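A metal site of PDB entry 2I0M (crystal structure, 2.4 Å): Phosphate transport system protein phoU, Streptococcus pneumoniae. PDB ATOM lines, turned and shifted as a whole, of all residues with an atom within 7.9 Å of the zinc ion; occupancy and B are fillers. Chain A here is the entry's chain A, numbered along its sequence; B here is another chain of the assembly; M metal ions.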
ATOM      1  N   MET A 129       3.962  12.390  19.817  1.00  0.00           N
ATOM      2  CA  MET A 129       3.388  12.348  21.159  1.00  0.00           C
ATOM      3  C   MET A 129       4.473  12.410  22.227  1.00  0.00           C
ATOM      4  O   MET A 129       4.354  13.181  23.178  1.00  0.00           O
ATOM      5  CB  MET A 129       2.517  11.102  21.351  1.00  0.00           C
ATOM      6  CG  MET A 129       1.035  11.209  20.881  1.00  0.00           C
ATOM      7  SD  MET A 129       0.168   9.582  20.900  1.00  0.00           S
ATOM      8  CE  MET A 129      -0.109   9.401  22.649  1.00  0.00           C
ATOM      9  N   ALA A 149      -2.351  13.114  25.662  1.00  0.00           N
ATOM     10  CA  ALA A 149      -3.014  11.843  26.002  1.00  0.00           C
ATOM     11  C   ALA A 149      -4.149  11.522  25.043  1.00  0.00           C
ATOM     12  O   ALA A 149      -4.331  10.367  24.680  1.00  0.00           O
ATOM     13  CB  ALA A 149      -3.530  11.854  27.447  1.00  0.00           C
ATOM     14  N   LYS A 151      -4.541  12.126  21.873  1.00  0.00           N
ATOM     15  CA  LYS A 151      -4.094  11.584  20.586  1.00  0.00           C
ATOM     16  C   LYS A 151      -3.948  10.053  20.557  1.00  0.00           C
ATOM     17  O   LYS A 151      -3.825   9.468  19.497  1.00  0.00           O
ATOM     18  CB  LYS A 151      -2.786  12.247  20.135  1.00  0.00           C
ATOM     19  CG  LYS A 151      -2.953  13.707  19.798  1.00  0.00           C
ATOM     20  CD  LYS A 151      -1.614  14.341  19.458  1.00  0.00           C
ATOM     21  CE  LYS A 151      -1.793  15.797  19.055  1.00  0.00           C
ATOM     22  NZ  LYS A 151      -0.656  16.241  18.209  1.00  0.00           N
ATOM     23  N   ASP A 152      -3.973   9.437  21.736  1.00  0.00           N
ATOM     24  CA  ASP A 152      -3.960   7.972  21.848  1.00  0.00           C
ATOM     25  C   ASP A 152      -5.203   7.309  21.248  1.00  0.00           C
ATOM     26  O   ASP A 152      -5.113   6.195  20.750  1.00  0.00           O
ATOM     27  CB  ASP A 152      -3.775   7.536  23.306  1.00  0.00           C
ATOM     28  CG  ASP A 152      -3.398   6.069  23.442  1.00  0.00           C
ATOM     29  OD1 ASP A 152      -2.415   5.624  22.809  1.00  0.00           O
ATOM     30  OD2 ASP A 152      -4.088   5.366  24.183  1.00  0.00           O
ATOM     31  N   GLU A 153      -6.357   8.000  21.300  1.00  0.00           N
ATOM     32  CA  GLU A 153      -7.551   7.563  20.571  1.00  0.00           C
ATOM     33  C   GLU A 153      -7.204   7.200  19.123  1.00  0.00           C
ATOM     34  O   GLU A 153      -7.565   6.131  18.653  1.00  0.00           O
ATOM     35  CB  GLU A 153      -8.675   8.636  20.588  1.00  0.00           C
ATOM     36  CG  GLU A 153     -10.096   8.065  20.379  1.00  0.00           C
ATOM     37  CD  GLU A 153     -11.193   9.139  20.130  1.00  0.00           C
ATOM     38  OE1 GLU A 153     -10.952  10.347  20.345  1.00  0.00           O
ATOM     39  OE2 GLU A 153     -12.308   8.761  19.714  1.00  0.00           O
ATOM     40  N   GLN A 154      -6.456   8.075  18.450  1.00  0.00           N
ATOM     41  CA  GLN A 154      -6.038   7.836  17.062  1.00  0.00           C
ATOM     42  C   GLN A 154      -5.122   6.614  16.886  1.00  0.00           C
ATOM     43  O   GLN A 154      -5.276   5.861  15.915  1.00  0.00           O
ATOM     44  CB  GLN A 154      -5.387   9.076  16.457  1.00  0.00           C
ATOM     45  CG  GLN A 154      -6.359  10.146  16.028  1.00  0.00           C
ATOM     46  CD  GLN A 154      -6.544  11.235  17.067  1.00  0.00           C
ATOM     47  OE1 GLN A 154      -7.548  11.252  17.792  1.00  0.00           O
ATOM     48  NE2 GLN A 154      -5.583  12.160  17.139  1.00  0.00           N
ATOM     49  N   ILE A 155      -4.186   6.438  17.808  1.00  0.00           N
ATOM     50  CA  ILE A 155      -3.301   5.275  17.794  1.00  0.00           C
ATOM     51  C   ILE A 155      -4.063   3.962  17.960  1.00  0.00           C
ATOM     52  O   ILE A 155      -3.765   2.979  17.279  1.00  0.00           O
ATOM     53  CB  ILE A 155      -2.090   5.453  18.734  1.00  0.00           C
ATOM     54  CG1 ILE A 155      -0.986   6.179  17.963  1.00  0.00           C
ATOM     55  CG2 ILE A 155      -1.549   4.124  19.234  1.00  0.00           C
ATOM     56  CD1 ILE A 155      -0.117   6.983  18.774  1.00  0.00           C
ATOM     57  N   ASP A 156      -5.067   3.967  18.840  1.00  0.00           N
ATOM     58  CA  ASP A 156      -5.990   2.855  18.993  1.00  0.00           C
ATOM     59  C   ASP A 156      -6.723   2.537  17.684  1.00  0.00           C
ATOM     60  O   ASP A 156      -6.865   1.368  17.318  1.00  0.00           O
ATOM     61  CB  ASP A 156      -6.993   3.138  20.120  1.00  0.00           C
ATOM     62  CG  ASP A 156      -6.369   2.955  21.506  1.00  0.00           C
ATOM     63  OD1 ASP A 156      -7.030   3.331  22.509  1.00  0.00           O
ATOM     64  OD2 ASP A 156      -5.229   2.444  21.596  1.00  0.00           O
ATOM     65  N   GLN A 157      -7.171   3.584  16.987  1.00  0.00           N
ATOM     66  CA  GLN A 157      -7.825   3.442  15.683  1.00  0.00           C
ATOM     67  C   GLN A 157      -6.873   2.840  14.646  1.00  0.00           C
ATOM     68  O   GLN A 157      -7.253   1.942  13.899  1.00  0.00           O
ATOM     69  CB  GLN A 157      -8.365   4.783  15.213  1.00  0.00           C
ATOM     70  CG  GLN A 157      -9.553   5.261  16.031  1.00  0.00           C
ATOM     71  CD  GLN A 157      -9.919   6.729  15.788  1.00  0.00           C
ATOM     72  OE1 GLN A 157     -10.699   7.305  16.555  1.00  0.00           O
ATOM     73  NE2 GLN A 157      -9.386   7.328  14.724  1.00  0.00           N
ATOM     74  N   TYR A 159      -4.409   0.985  15.547  1.00  0.00           N
ATOM     75  CA  TYR A 159      -4.217  -0.363  16.063  1.00  0.00           C
ATOM     76  C   TYR A 159      -5.273  -1.355  15.539  1.00  0.00           C
ATOM     77  O   TYR A 159      -4.923  -2.440  15.070  1.00  0.00           O
ATOM     78  CB  TYR A 159      -4.157  -0.376  17.601  1.00  0.00           C
ATOM     79  CG  TYR A 159      -3.983  -1.756  18.169  1.00  0.00           C
ATOM     80  CD1 TYR A 159      -2.797  -2.449  17.987  1.00  0.00           C
ATOM     81  CD2 TYR A 159      -5.011  -2.374  18.867  1.00  0.00           C
ATOM     82  CE1 TYR A 159      -2.626  -3.736  18.471  1.00  0.00           C
ATOM     83  CE2 TYR A 159      -4.844  -3.671  19.371  1.00  0.00           C
ATOM     84  CZ  TYR A 159      -3.640  -4.337  19.166  1.00  0.00           C
ATOM     85  OH  TYR A 159      -3.455  -5.610  19.660  1.00  0.00           O
ATOM     86  N   TYR A 160      -6.549  -0.995  15.615  1.00  0.00           N
ATOM     87  CA  TYR A 160      -7.610  -1.904  15.214  1.00  0.00           C
ATOM     88  C   TYR A 160      -7.715  -2.064  13.701  1.00  0.00           C
ATOM     89  O   TYR A 160      -7.814  -3.190  13.215  1.00  0.00           O
ATOM     90  CB  TYR A 160      -8.950  -1.538  15.873  1.00  0.00           C
ATOM     91  CG  TYR A 160      -8.938  -1.766  17.385  1.00  0.00           C
ATOM     92  CD1 TYR A 160      -8.971  -3.061  17.924  1.00  0.00           C
ATOM     93  CD2 TYR A 160      -8.847  -0.690  18.265  1.00  0.00           C
ATOM     94  CE1 TYR A 160      -8.946  -3.265  19.304  1.00  0.00           C
ATOM     95  CE2 TYR A 160      -8.809  -0.879  19.654  1.00  0.00           C
ATOM     96  CZ  TYR A 160      -8.854  -2.167  20.159  1.00  0.00           C
ATOM     97  OH  TYR A 160      -8.820  -2.358  21.527  1.00  0.00           O
ATOM     98  N   LEU A 190       3.727  -0.498  19.440  1.00  0.00           N
ATOM     99  CA  LEU A 190       3.457   0.919  19.246  1.00  0.00           C
ATOM    100  C   LEU A 190       2.253   1.345  20.061  1.00  0.00           C
ATOM    101  O   LEU A 190       2.256   2.430  20.647  1.00  0.00           O
ATOM    102  CB  LEU A 190       3.193   1.231  17.756  1.00  0.00           C
ATOM    103  CG  LEU A 190       4.389   1.471  16.844  1.00  0.00           C
ATOM    104  CD1 LEU A 190       3.958   1.617  15.394  1.00  0.00           C
ATOM    105  CD2 LEU A 190       5.155   2.705  17.318  1.00  0.00           C
ATOM    106  N   GLU A 191       1.228   0.501  20.084  1.00  0.00           N
ATOM    107  CA  GLU A 191       0.032   0.804  20.832  1.00  0.00           C
ATOM    108  C   GLU A 191       0.371   0.919  22.338  1.00  0.00           C
ATOM    109  O   GLU A 191      -0.085   1.873  22.984  1.00  0.00           O
ATOM    110  CB  GLU A 191      -1.074  -0.228  20.545  1.00  0.00           C
ATOM    111  CG  GLU A 191      -2.479   0.173  21.009  1.00  0.00           C
ATOM    112  CD  GLU A 191      -2.675   0.072  22.522  1.00  0.00           C
ATOM    113  OE1 GLU A 191      -2.022  -0.791  23.161  1.00  0.00           O
ATOM    114  OE2 GLU A 191      -3.484   0.843  23.080  1.00  0.00           O
ATOM    115  N   ARG A 192       1.173  -0.012  22.879  1.00  0.00           N
ATOM    116  CA  ARG A 192       1.667   0.044  24.267  1.00  0.00           C
ATOM    117  C   ARG A 192       2.560   1.243  24.563  1.00  0.00           C
ATOM    118  O   ARG A 192       2.369   1.913  25.580  1.00  0.00           O
ATOM    119  CB  ARG A 192       2.440  -1.233  24.649  1.00  0.00           C
ATOM    120  CG  ARG A 192       1.667  -2.502  24.585  1.00  0.00           C
ATOM    121  CD  ARG A 192       0.608  -2.554  25.663  1.00  0.00           C
ATOM    122  NE  ARG A 192       1.148  -3.044  26.927  1.00  0.00           N
ATOM    123  CZ  ARG A 192       1.624  -2.259  27.890  1.00  0.00           C
ATOM    124  NH1 ARG A 192       1.610  -0.933  27.738  1.00  0.00           N
ATOM    125  NH2 ARG A 192       2.087  -2.785  29.003  1.00  0.00           N
ATOM    126  N   PHE A 193       3.536   1.491  23.694  1.00  0.00           N
ATOM    127  CA  PHE A 193       4.370   2.699  23.718  1.00  0.00           C
ATOM    128  C   PHE A 193       3.534   3.941  23.976  1.00  0.00           C
ATOM    129  O   PHE A 193       3.812   4.716  24.880  1.00  0.00           O
ATOM    130  CB  PHE A 193       5.105   2.829  22.379  1.00  0.00           C
ATOM    131  CG  PHE A 193       6.107   3.941  22.321  1.00  0.00           C
ATOM    132  CD1 PHE A 193       7.401   3.775  22.800  1.00  0.00           C
ATOM    133  CD2 PHE A 193       5.781   5.141  21.704  1.00  0.00           C
ATOM    134  CE1 PHE A 193       8.344   4.807  22.690  1.00  0.00           C
ATOM    135  CE2 PHE A 193       6.716   6.179  21.595  1.00  0.00           C
ATOM    136  CZ  PHE A 193       8.006   6.004  22.094  1.00  0.00           C
ATOM    137  N   ALA A 194       2.491   4.110  23.168  1.00  0.00           N
ATOM    138  CA  ALA A 194       1.625   5.283  23.241  1.00  0.00           C
ATOM    139  C   ALA A 194       0.761   5.314  24.494  1.00  0.00           C
ATOM    140  O   ALA A 194       0.496   6.376  25.053  1.00  0.00           O
ATOM    141  CB  ALA A 194       0.763   5.390  21.975  1.00  0.00           C
ATOM    142  N   ASP A 195       0.327   4.144  24.955  1.00  0.00           N
ATOM    143  CA  ASP A 195      -0.379   4.033  26.218  1.00  0.00           C
ATOM    144  C   ASP A 195       0.467   4.533  27.396  1.00  0.00           C
ATOM    145  O   ASP A 195      -0.039   5.275  28.239  1.00  0.00           O
ATOM    146  CB  ASP A 195      -0.790   2.582  26.445  1.00  0.00           C
ATOM    147  CG  ASP A 195      -2.163   2.262  25.881  1.00  0.00           C
ATOM    148  OD1 ASP A 195      -2.935   3.202  25.594  1.00  0.00           O
ATOM    149  OD2 ASP A 195      -2.479   1.046  25.736  1.00  0.00           O
ATOM    150  N   TYR A 196       1.736   4.120  27.476  1.00  0.00           N
ATOM    151  CA  TYR A 196       2.624   4.647  28.530  1.00  0.00           C
ATOM    152  C   TYR A 196       2.813   6.170  28.502  1.00  0.00           C
ATOM    153  O   TYR A 196       2.869   6.801  29.565  1.00  0.00           O
ATOM    154  CB  TYR A 196       3.987   3.946  28.542  1.00  0.00           C
ATOM    155  CG  TYR A 196       3.929   2.527  29.058  1.00  0.00           C
ATOM    156  CD1 TYR A 196       3.552   2.253  30.372  1.00  0.00           C
ATOM    157  CD2 TYR A 196       4.223   1.440  28.221  1.00  0.00           C
ATOM    158  CE1 TYR A 196       3.475   0.929  30.862  1.00  0.00           C
ATOM    159  CE2 TYR A 196       4.138   0.124  28.699  1.00  0.00           C
ATOM    160  CZ  TYR A 196       3.776  -0.116  30.012  1.00  0.00           C
ATOM    161  OH  TYR A 196       3.710  -1.407  30.480  1.00  0.00           O
ATOM    162  N   ALA A 198       0.536   8.244  27.586  1.00  0.00           N
ATOM    163  CA  ALA A 198      -0.716   8.701  28.163  1.00  0.00           C
ATOM    164  C   ALA A 198      -0.683   8.593  29.689  1.00  0.00           C
ATOM    165  O   ALA A 198      -1.113   9.504  30.392  1.00  0.00           O
ATOM    166  CB  ALA A 198      -1.895   7.889  27.578  1.00  0.00           C
ATOM    167  N   ARG B 192      -3.643  -6.774  28.996  1.00  0.00           N
ATOM    168  CA  ARG B 192      -2.934  -5.726  29.759  1.00  0.00           C
ATOM    169  C   ARG B 192      -2.832  -6.016  31.252  1.00  0.00           C
ATOM    170  O   ARG B 192      -1.758  -5.880  31.837  1.00  0.00           O
ATOM    171  CB  ARG B 192      -3.596  -4.351  29.590  1.00  0.00           C
ATOM    172  CG  ARG B 192      -3.627  -3.814  28.195  1.00  0.00           C
ATOM    173  CD  ARG B 192      -2.243  -3.468  27.713  1.00  0.00           C
ATOM    174  NE  ARG B 192      -1.847  -2.119  28.121  1.00  0.00           N
ATOM    175  CZ  ARG B 192      -1.173  -1.854  29.240  1.00  0.00           C
ATOM    176  NH1 ARG B 192      -0.794  -2.847  30.048  1.00  0.00           N
ATOM    177  NH2 ARG B 192      -0.850  -0.607  29.528  1.00  0.00           N
HETATM  178 ZN    ZN M   1      -3.845   2.799  23.275  1.00  0.00          ZN
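Four residues have an atom within 4 Å of the zinc ion: Asp 152, Asp 156, Glu 191 and Asp 195. The nearest printed residue that does not touch the zinc ion is Ile 155 (4.8 Å).
The zinc ion is bound by OE2 of Glu 191, OD2 of Asp 156 and OD1 of Asp 195. Slightly farther from the zinc ion lies OD2 of Asp 152 (2.7 Å).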
